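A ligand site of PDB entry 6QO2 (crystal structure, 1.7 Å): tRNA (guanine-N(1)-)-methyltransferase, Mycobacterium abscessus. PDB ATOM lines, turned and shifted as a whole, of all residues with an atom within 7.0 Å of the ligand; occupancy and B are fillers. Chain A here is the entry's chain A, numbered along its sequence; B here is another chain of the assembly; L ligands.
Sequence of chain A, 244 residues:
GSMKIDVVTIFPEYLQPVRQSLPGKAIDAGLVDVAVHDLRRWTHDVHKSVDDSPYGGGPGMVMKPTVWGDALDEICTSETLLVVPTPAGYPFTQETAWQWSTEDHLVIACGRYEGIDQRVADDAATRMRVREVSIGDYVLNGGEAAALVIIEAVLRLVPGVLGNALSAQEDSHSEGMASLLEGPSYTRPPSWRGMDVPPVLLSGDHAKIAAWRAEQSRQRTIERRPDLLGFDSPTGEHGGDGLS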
ATOM      1  N   VAL A  84      -2.711   4.141   5.928  1.00  0.00           N
ATOM      2  CA  VAL A  84      -1.277   3.949   5.736  1.00  0.00           C
ATOM      3  C   VAL A  84      -0.931   4.222   4.278  1.00  0.00           C
ATOM      4  O   VAL A  84      -1.140   3.372   3.412  1.00  0.00           O
ATOM      5  CB  VAL A  84      -0.809   2.530   6.117  1.00  0.00           C
ATOM      6  CG1 VAL A  84       0.713   2.422   6.003  1.00  0.00           C
ATOM      7  CG2 VAL A  84      -1.279   2.162   7.521  1.00  0.00           C
ATOM      8  N   PRO A  85      -0.412   5.427   3.991  1.00  0.00           N
ATOM      9  CA  PRO A  85       0.004   5.693   2.615  1.00  0.00           C
ATOM     10  C   PRO A  85       1.153   4.788   2.199  1.00  0.00           C
ATOM     11  O   PRO A  85       2.110   4.572   2.952  1.00  0.00           O
ATOM     12  CB  PRO A  85       0.422   7.170   2.648  1.00  0.00           C
ATOM     13  CG  PRO A  85      -0.351   7.759   3.821  1.00  0.00           C
ATOM     14  CD  PRO A  85      -0.410   6.640   4.836  1.00  0.00           C
ATOM     15  N   THR A  86       1.045   4.217   1.003  1.00  0.00           N
ATOM     16  CA  THR A  86       2.091   3.337   0.488  1.00  0.00           C
ATOM     17  C   THR A  86       1.921   3.190  -1.010  1.00  0.00           C
ATOM     18  O   THR A  86       0.805   3.144  -1.497  1.00  0.00           O
ATOM     19  CB  THR A  86       2.081   1.945   1.169  1.00  0.00           C
ATOM     20  OG1 THR A  86       2.852   1.021   0.386  1.00  0.00           O
ATOM     21  CG2 THR A  86       0.682   1.407   1.370  1.00  0.00           C
ATOM     22  N   PRO A  87       3.032   3.130  -1.750  1.00  0.00           N
ATOM     23  CA  PRO A  87       2.890   2.955  -3.200  1.00  0.00           C
ATOM     24  C   PRO A  87       2.249   1.606  -3.541  1.00  0.00           C
ATOM     25  O   PRO A  87       1.783   1.434  -4.670  1.00  0.00           O
ATOM     26  CB  PRO A  87       4.337   3.019  -3.711  1.00  0.00           C
ATOM     27  CG  PRO A  87       5.183   2.666  -2.508  1.00  0.00           C
ATOM     28  CD  PRO A  87       4.432   3.215  -1.328  1.00  0.00           C
ATOM     29  N   ALA A  88       2.246   0.689  -2.587  1.00  0.00           N
ATOM     30  CA  ALA A  88       1.651  -0.636  -2.792  1.00  0.00           C
ATOM     31  C   ALA A  88       0.197  -0.682  -2.332  1.00  0.00           C
ATOM     32  O   ALA A  88      -0.372  -1.761  -2.172  1.00  0.00           O
ATOM     33  CB  ALA A  88       2.454  -1.698  -2.045  1.00  0.00           C
ATOM     34  N   GLY A  89      -0.411   0.480  -2.117  1.00  0.00           N
ATOM     35  CA  GLY A  89      -1.755   0.490  -1.570  1.00  0.00           C
ATOM     36  C   GLY A  89      -2.846   0.367  -2.603  1.00  0.00           C
ATOM     37  O   GLY A  89      -2.603   0.399  -3.812  1.00  0.00           O
ATOM     38  N   ALA A 109      -0.597   7.094   9.264  1.00  0.00           N
ATOM     39  CA  ALA A 109       0.753   6.646   9.620  1.00  0.00           C
ATOM     40  C   ALA A 109       1.681   6.854   8.455  1.00  0.00           C
ATOM     41  O   ALA A 109       1.603   6.127   7.460  1.00  0.00           O
ATOM     42  CB  ALA A 109       0.730   5.180  10.012  1.00  0.00           C
ATOM     43  N   CYS A 110       2.591   7.818   8.578  1.00  0.00           N
ATOM     44  CA  CYS A 110       3.493   8.166   7.484  1.00  0.00           C
ATOM     45  C   CYS A 110       4.786   7.372   7.532  1.00  0.00           C
ATOM     46  O   CYS A 110       5.572   7.513   8.471  1.00  0.00           O
ATOM     47  CB  CYS A 110       3.809   9.659   7.519  1.00  0.00           C
ATOM     48  SG  CYS A 110       2.394  10.716   7.291  1.00  0.00           S
ATOM     49  N   GLY A 111       5.002   6.545   6.523  1.00  0.00           N
ATOM     50  CA  GLY A 111       6.219   5.767   6.448  1.00  0.00           C
ATOM     51  C   GLY A 111       7.331   6.447   5.675  1.00  0.00           C
ATOM     52  O   GLY A 111       7.084   7.388   4.912  1.00  0.00           O
ATOM     53  N   ARG A 112       8.543   5.962   5.888  1.00  0.00           N
ATOM     54  CA  ARG A 112       9.742   6.426   5.189  1.00  0.00           C
ATOM     55  C   ARG A 112      10.596   5.211   4.834  1.00  0.00           C
ATOM     56  O   ARG A 112      10.204   4.069   5.104  1.00  0.00           O
ATOM     57  CB  ARG A 112      10.540   7.417   6.051  1.00  0.00           C
ATOM     58  CG  ARG A 112       9.964   8.838   6.106  1.00  0.00           C
ATOM     59  CD  ARG A 112      10.644   9.759   5.089  1.00  0.00           C
ATOM     60  NE  ARG A 112       9.766  10.843   4.643  1.00  0.00           N
ATOM     61  CZ  ARG A 112      10.136  11.815   3.814  1.00  0.00           C
ATOM     62  NH1 ARG A 112      11.376  11.853   3.339  1.00  0.00           N
ATOM     63  NH2 ARG A 112       9.262  12.760   3.451  1.00  0.00           N
ATOM     64  N   TYR A 113      11.765   5.454   4.243  1.00  0.00           N
ATOM     65  CA  TYR A 113      12.623   4.358   3.785  1.00  0.00           C
ATOM     66  C   TYR A 113      11.820   3.416   2.893  1.00  0.00           C
ATOM     67  O   TYR A 113      11.101   3.859   2.006  1.00  0.00           O
ATOM     68  CB  TYR A 113      13.227   3.605   4.964  1.00  0.00           C
ATOM     69  CG  TYR A 113      13.806   4.471   6.057  1.00  0.00           C
ATOM     70  CD1 TYR A 113      15.126   4.898   6.008  1.00  0.00           C
ATOM     71  CD2 TYR A 113      13.030   4.849   7.142  1.00  0.00           C
ATOM     72  CE1 TYR A 113      15.656   5.681   7.008  1.00  0.00           C
ATOM     73  CE2 TYR A 113      13.551   5.631   8.153  1.00  0.00           C
ATOM     74  CZ  TYR A 113      14.869   6.048   8.085  1.00  0.00           C
ATOM     75  OH  TYR A 113      15.379   6.830   9.086  1.00  0.00           O
ATOM     76  N   GLY A 115       9.371   1.301   3.876  1.00  0.00           N
ATOM     77  CA  GLY A 115       8.058   0.971   4.415  1.00  0.00           C
ATOM     78  C   GLY A 115       8.070   0.632   5.901  1.00  0.00           C
ATOM     79  O   GLY A 115       9.115   0.607   6.519  1.00  0.00           O
ATOM     80  N   VAL A 133      -3.201   2.748   1.237  1.00  0.00           N
ATOM     81  CA  VAL A 133      -3.608   3.417  -0.005  1.00  0.00           C
ATOM     82  C   VAL A 133      -2.487   4.138  -0.689  1.00  0.00           C
ATOM     83  O   VAL A 133      -1.558   4.641  -0.046  1.00  0.00           O
ATOM     84  CB  VAL A 133      -4.743   4.461   0.236  1.00  0.00           C
ATOM     85  CG1 VAL A 133      -6.038   3.760   0.659  1.00  0.00           C
ATOM     86  CG2 VAL A 133      -4.312   5.531   1.252  1.00  0.00           C
ATOM     87  N   SER A 134      -2.572   4.187  -2.020  1.00  0.00           N
ATOM     88  CA  SER A 134      -1.673   4.989  -2.850  1.00  0.00           C
ATOM     89  C   SER A 134      -2.410   6.185  -3.436  1.00  0.00           C
ATOM     90  O   SER A 134      -3.572   6.069  -3.816  1.00  0.00           O
ATOM     91  CB  SER A 134      -1.088   4.143  -3.984  1.00  0.00           C
ATOM     92  OG  SER A 134      -0.523   4.960  -4.985  1.00  0.00           O
ATOM     93  N   ILE A 135      -1.746   7.338  -3.538  1.00  0.00           N
ATOM     94  CA  ILE A 135      -2.412   8.518  -4.113  1.00  0.00           C
ATOM     95  C   ILE A 135      -2.115   8.668  -5.593  1.00  0.00           C
ATOM     96  O   ILE A 135      -2.649   9.561  -6.249  1.00  0.00           O
ATOM     97  CB  ILE A 135      -2.025   9.842  -3.388  1.00  0.00           C
ATOM     98  CG1 ILE A 135      -0.523  10.135  -3.476  1.00  0.00           C
ATOM     99  CG2 ILE A 135      -2.521   9.824  -1.936  1.00  0.00           C
ATOM    100  CD1 ILE A 135      -0.177  11.613  -3.122  1.00  0.00           C
ATOM    101  N   GLY A 136      -1.264   7.801  -6.124  1.00  0.00           N
ATOM    102  CA  GLY A 136      -0.986   7.831  -7.549  1.00  0.00           C
ATOM    103  C   GLY A 136       0.199   6.968  -7.901  1.00  0.00           C
ATOM    104  O   GLY A 136       0.880   6.444  -7.017  1.00  0.00           O
ATOM    105  N   ASP A 137       0.439   6.789  -9.196  1.00  0.00           N
ATOM    106  CA  ASP A 137       1.507   5.900  -9.613  1.00  0.00           C
ATOM    107  C   ASP A 137       2.831   6.615  -9.798  1.00  0.00           C
ATOM    108  O   ASP A 137       3.302   6.797 -10.917  1.00  0.00           O
ATOM    109  CB  ASP A 137       1.131   5.179 -10.905  1.00  0.00           C
ATOM    110  CG  ASP A 137       0.000   4.201 -10.698  1.00  0.00           C
ATOM    111  OD1 ASP A 137      -0.127   3.681  -9.575  1.00  0.00           O
ATOM    112  OD2 ASP A 137      -0.755   3.940 -11.659  1.00  0.00           O
ATOM    113  N   TYR A 138       3.408   7.032  -8.678  1.00  0.00           N
ATOM    114  CA  TYR A 138       4.701   7.669  -8.646  1.00  0.00           C
ATOM    115  C   TYR A 138       5.263   7.367  -7.278  1.00  0.00           C
ATOM    116  O   TYR A 138       4.532   7.033  -6.346  1.00  0.00           O
ATOM    117  CB  TYR A 138       4.631   9.184  -8.876  1.00  0.00           C
ATOM    118  CG  TYR A 138       3.389   9.808  -8.312  1.00  0.00           C
ATOM    119  CD1 TYR A 138       3.249  10.002  -6.938  1.00  0.00           C
ATOM    120  CD2 TYR A 138       2.318  10.159  -9.135  1.00  0.00           C
ATOM    121  CE1 TYR A 138       2.086  10.538  -6.412  1.00  0.00           C
ATOM    122  CE2 TYR A 138       1.165  10.705  -8.610  1.00  0.00           C
ATOM    123  CZ  TYR A 138       1.054  10.890  -7.250  1.00  0.00           C
ATOM    124  OH  TYR A 138      -0.099  11.427  -6.715  1.00  0.00           O
ATOM    125  N   VAL A 139       6.571   7.495  -7.179  1.00  0.00           N
ATOM    126  CA  VAL A 139       7.259   7.196  -5.927  1.00  0.00           C
ATOM    127  C   VAL A 139       7.647   8.471  -5.212  1.00  0.00           C
ATOM    128  O   VAL A 139       8.272   9.356  -5.788  1.00  0.00           O
ATOM    129  CB  VAL A 139       8.537   6.368  -6.180  1.00  0.00           C
ATOM    130  CG1 VAL A 139       9.205   6.009  -4.865  1.00  0.00           C
ATOM    131  CG2 VAL A 139       8.208   5.124  -6.984  1.00  0.00           C
ATOM    132  N   LEU A 140       7.257   8.554  -3.936  1.00  0.00           N
ATOM    133  CA  LEU A 140       7.666   9.661  -3.089  1.00  0.00           C
ATOM    134  C   LEU A 140       8.766   9.163  -2.147  1.00  0.00           C
ATOM    135  O   LEU A 140       8.990   7.961  -2.052  1.00  0.00           O
ATOM    136  CB  LEU A 140       6.476  10.190  -2.288  1.00  0.00           C
ATOM    137  CG  LEU A 140       5.232  10.485  -3.139  1.00  0.00           C
ATOM    138  CD1 LEU A 140       4.027  10.804  -2.282  1.00  0.00           C
ATOM    139  CD2 LEU A 140       5.529  11.623  -4.103  1.00  0.00           C
ATOM    140  N   ASN A 141       9.419  10.067  -1.427  1.00  0.00           N
ATOM    141  CA  ASN A 141      10.384   9.635  -0.419  1.00  0.00           C
ATOM    142  C   ASN A 141       9.720   9.088   0.831  1.00  0.00           C
ATOM    143  O   ASN A 141      10.294   8.298   1.591  1.00  0.00           O
ATOM    144  CB  ASN A 141      11.311  10.784  -0.029  1.00  0.00           C
ATOM    145  CG  ASN A 141      12.374  11.038  -1.071  1.00  0.00           C
ATOM    146  OD1 ASN A 141      12.895  10.107  -1.682  1.00  0.00           O
ATOM    147  ND2 ASN A 141      12.709  12.308  -1.276  1.00  0.00           N
ATOM    148  N   GLY A 142       8.486   9.507   1.075  1.00  0.00           N
ATOM    149  CA  GLY A 142       7.812   9.099   2.284  1.00  0.00           C
ATOM    150  C   GLY A 142       6.358   9.467   2.203  1.00  0.00           C
ATOM    151  O   GLY A 142       5.933  10.049   1.207  1.00  0.00           O
ATOM    152  N   GLY A 143       5.589   9.133   3.240  1.00  0.00           N
ATOM    153  CA  GLY A 143       4.146   9.291   3.192  1.00  0.00           C
ATOM    154  C   GLY A 143       3.599  10.677   3.466  1.00  0.00           C
ATOM    155  O   GLY A 143       2.400  10.883   3.367  1.00  0.00           O
ATOM    156  N   GLU A 144       4.455  11.633   3.808  1.00  0.00           N
ATOM    157  CA  GLU A 144       3.956  12.932   4.289  1.00  0.00           C
ATOM    158  C   GLU A 144       3.182  13.701   3.211  1.00  0.00           C
ATOM    159  O   GLU A 144       2.117  14.257   3.472  1.00  0.00           O
ATOM    160  CB  GLU A 144       5.127  13.781   4.785  1.00  0.00           C
ATOM    161  CG  GLU A 144       5.681  13.359   6.135  1.00  0.00           C
ATOM    162  CD  GLU A 144       6.528  12.098   6.115  1.00  0.00           C
ATOM    163  OE1 GLU A 144       6.974  11.659   5.030  1.00  0.00           O
ATOM    164  OE2 GLU A 144       6.762  11.531   7.205  1.00  0.00           O
ATOM    165  N   ALA A 146       1.649  12.441   0.721  1.00  0.00           N
ATOM    166  CA  ALA A 146       0.418  11.694   0.512  1.00  0.00           C
ATOM    167  C   ALA A 146      -0.586  12.013   1.616  1.00  0.00           C
ATOM    168  O   ALA A 146      -1.771  12.158   1.366  1.00  0.00           O
ATOM    169  CB  ALA A 146       0.702  10.182   0.434  1.00  0.00           C
ATOM    170  N   VAL B 149       3.775  17.232  -4.271  1.00  0.00           N
ATOM    171  CA  VAL B 149       3.897  15.849  -4.725  1.00  0.00           C
ATOM    172  C   VAL B 149       4.818  15.785  -5.945  1.00  0.00           C
ATOM    173  O   VAL B 149       5.736  14.977  -6.002  1.00  0.00           O
ATOM    174  CB  VAL B 149       2.515  15.235  -5.068  1.00  0.00           C
ATOM    175  CG1 VAL B 149       2.650  13.948  -5.888  1.00  0.00           C
ATOM    176  CG2 VAL B 149       1.724  14.974  -3.788  1.00  0.00           C
ATOM    177  N   GLU B 152       8.536  16.471  -5.032  1.00  0.00           N
ATOM    178  CA  GLU B 152       9.162  15.342  -4.352  1.00  0.00           C
ATOM    179  C   GLU B 152       9.435  14.197  -5.322  1.00  0.00           C
ATOM    180  O   GLU B 152      10.525  13.616  -5.304  1.00  0.00           O
ATOM    181  CB  GLU B 152       8.293  14.866  -3.189  1.00  0.00           C
ATOM    182  CG  GLU B 152       8.829  13.613  -2.537  1.00  0.00           C
ATOM    183  CD  GLU B 152       8.323  13.474  -1.123  1.00  0.00           C
ATOM    184  OE1 GLU B 152       7.708  14.440  -0.611  1.00  0.00           O
ATOM    185  OE2 GLU B 152       8.513  12.388  -0.532  1.00  0.00           O
HETATM  186  C1  LIG L   1       4.384   6.383   1.372  1.00  0.00           C
HETATM  187  N1  LIG L   1       2.230   7.186  -4.526  1.00  0.00           N
HETATM  188  C2  LIG L   1       2.023   7.028  -3.137  1.00  0.00           C
HETATM  189  O1  LIG L   1       0.911   7.065  -2.659  1.00  0.00           O
HETATM  190  C3  LIG L   1       3.229   6.813  -2.243  1.00  0.00           C
HETATM  191  C4  LIG L   1       4.493   6.700  -2.819  1.00  0.00           C
HETATM  192  C5  LIG L   1       5.607   6.500  -2.015  1.00  0.00           C
HETATM  193  C6  LIG L   1       5.451   6.414  -0.604  1.00  0.00           C
HETATM  194  N2  LIG L   1       6.378   6.211   0.405  1.00  0.00           N
HETATM  195  C7  LIG L   1       5.738   6.194   1.592  1.00  0.00           C
HETATM  196  C8  LIG L   1       4.206   6.517  -0.040  1.00  0.00           C
HETATM  197  C9  LIG L   1       3.060   6.726  -0.861  1.00  0.00           C
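N of Gly 142 sits at hydrogen-bond distance from OE2 of Glu 152 of chain B (3.3 Å). The backbone carbonyl oxygen (O) of Gly 136 lies within hydrogen-bond range of the side-chain hydroxyl (OG) of Ser 134. The side-chain hydroxyl of Tyr 138 sits at hydrogen-bond distance from the backbone carbonyl oxygen of Ile 135 (3.2 Å). The backbone NH (N) of Gly 143 sits at hydrogen-bond distance from the backbone carbonyl oxygen (O) of Gly 111, at 2.8 Å. N of Thr 86 is in hydrogen-bond range of O of Val 133, at 2.8 Å. The side-chain hydroxyl of Thr 86 sits close to the backbone NH of Ala 88 (3.1 Å).
O1 of the ligand lies close to OG of Ser 134, at 3.4 Å. An oxygen (O1) of the ligand is in hydrogen-bond range of the backbone NH of Ile 135. The backbone carbonyl oxygen (O) of Tyr 138 sits at hydrogen-bond distance from a nitrogen (N1) of the ligand, 2.9 Å away. A nitrogen (N1) of the ligand is in hydrogen-bond range of the backbone carbonyl oxygen (O) of Gly 136, 2.9 Å away.
Pro 85 touches the ligand (O to C1, 3.3 Å). Thr 86 touches the ligand. Pro 87 touches the ligand (CD to C6, 3.4 Å). Gly 111 touches the ligand. Leu 140 touches the ligand. Gly 142 touches the ligand. Gly 143 touches the ligand. 11 residues have an atom within 4 Å of the ligand: Pro 85, Thr 86, Pro 87, Gly 111, Ser 134, Ile 135, Gly 136, Tyr 138, Leu 140, Gly 142 and Gly 143. The nearest printed residue that does not touch the ligand is Val 139 (4.2 Å).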
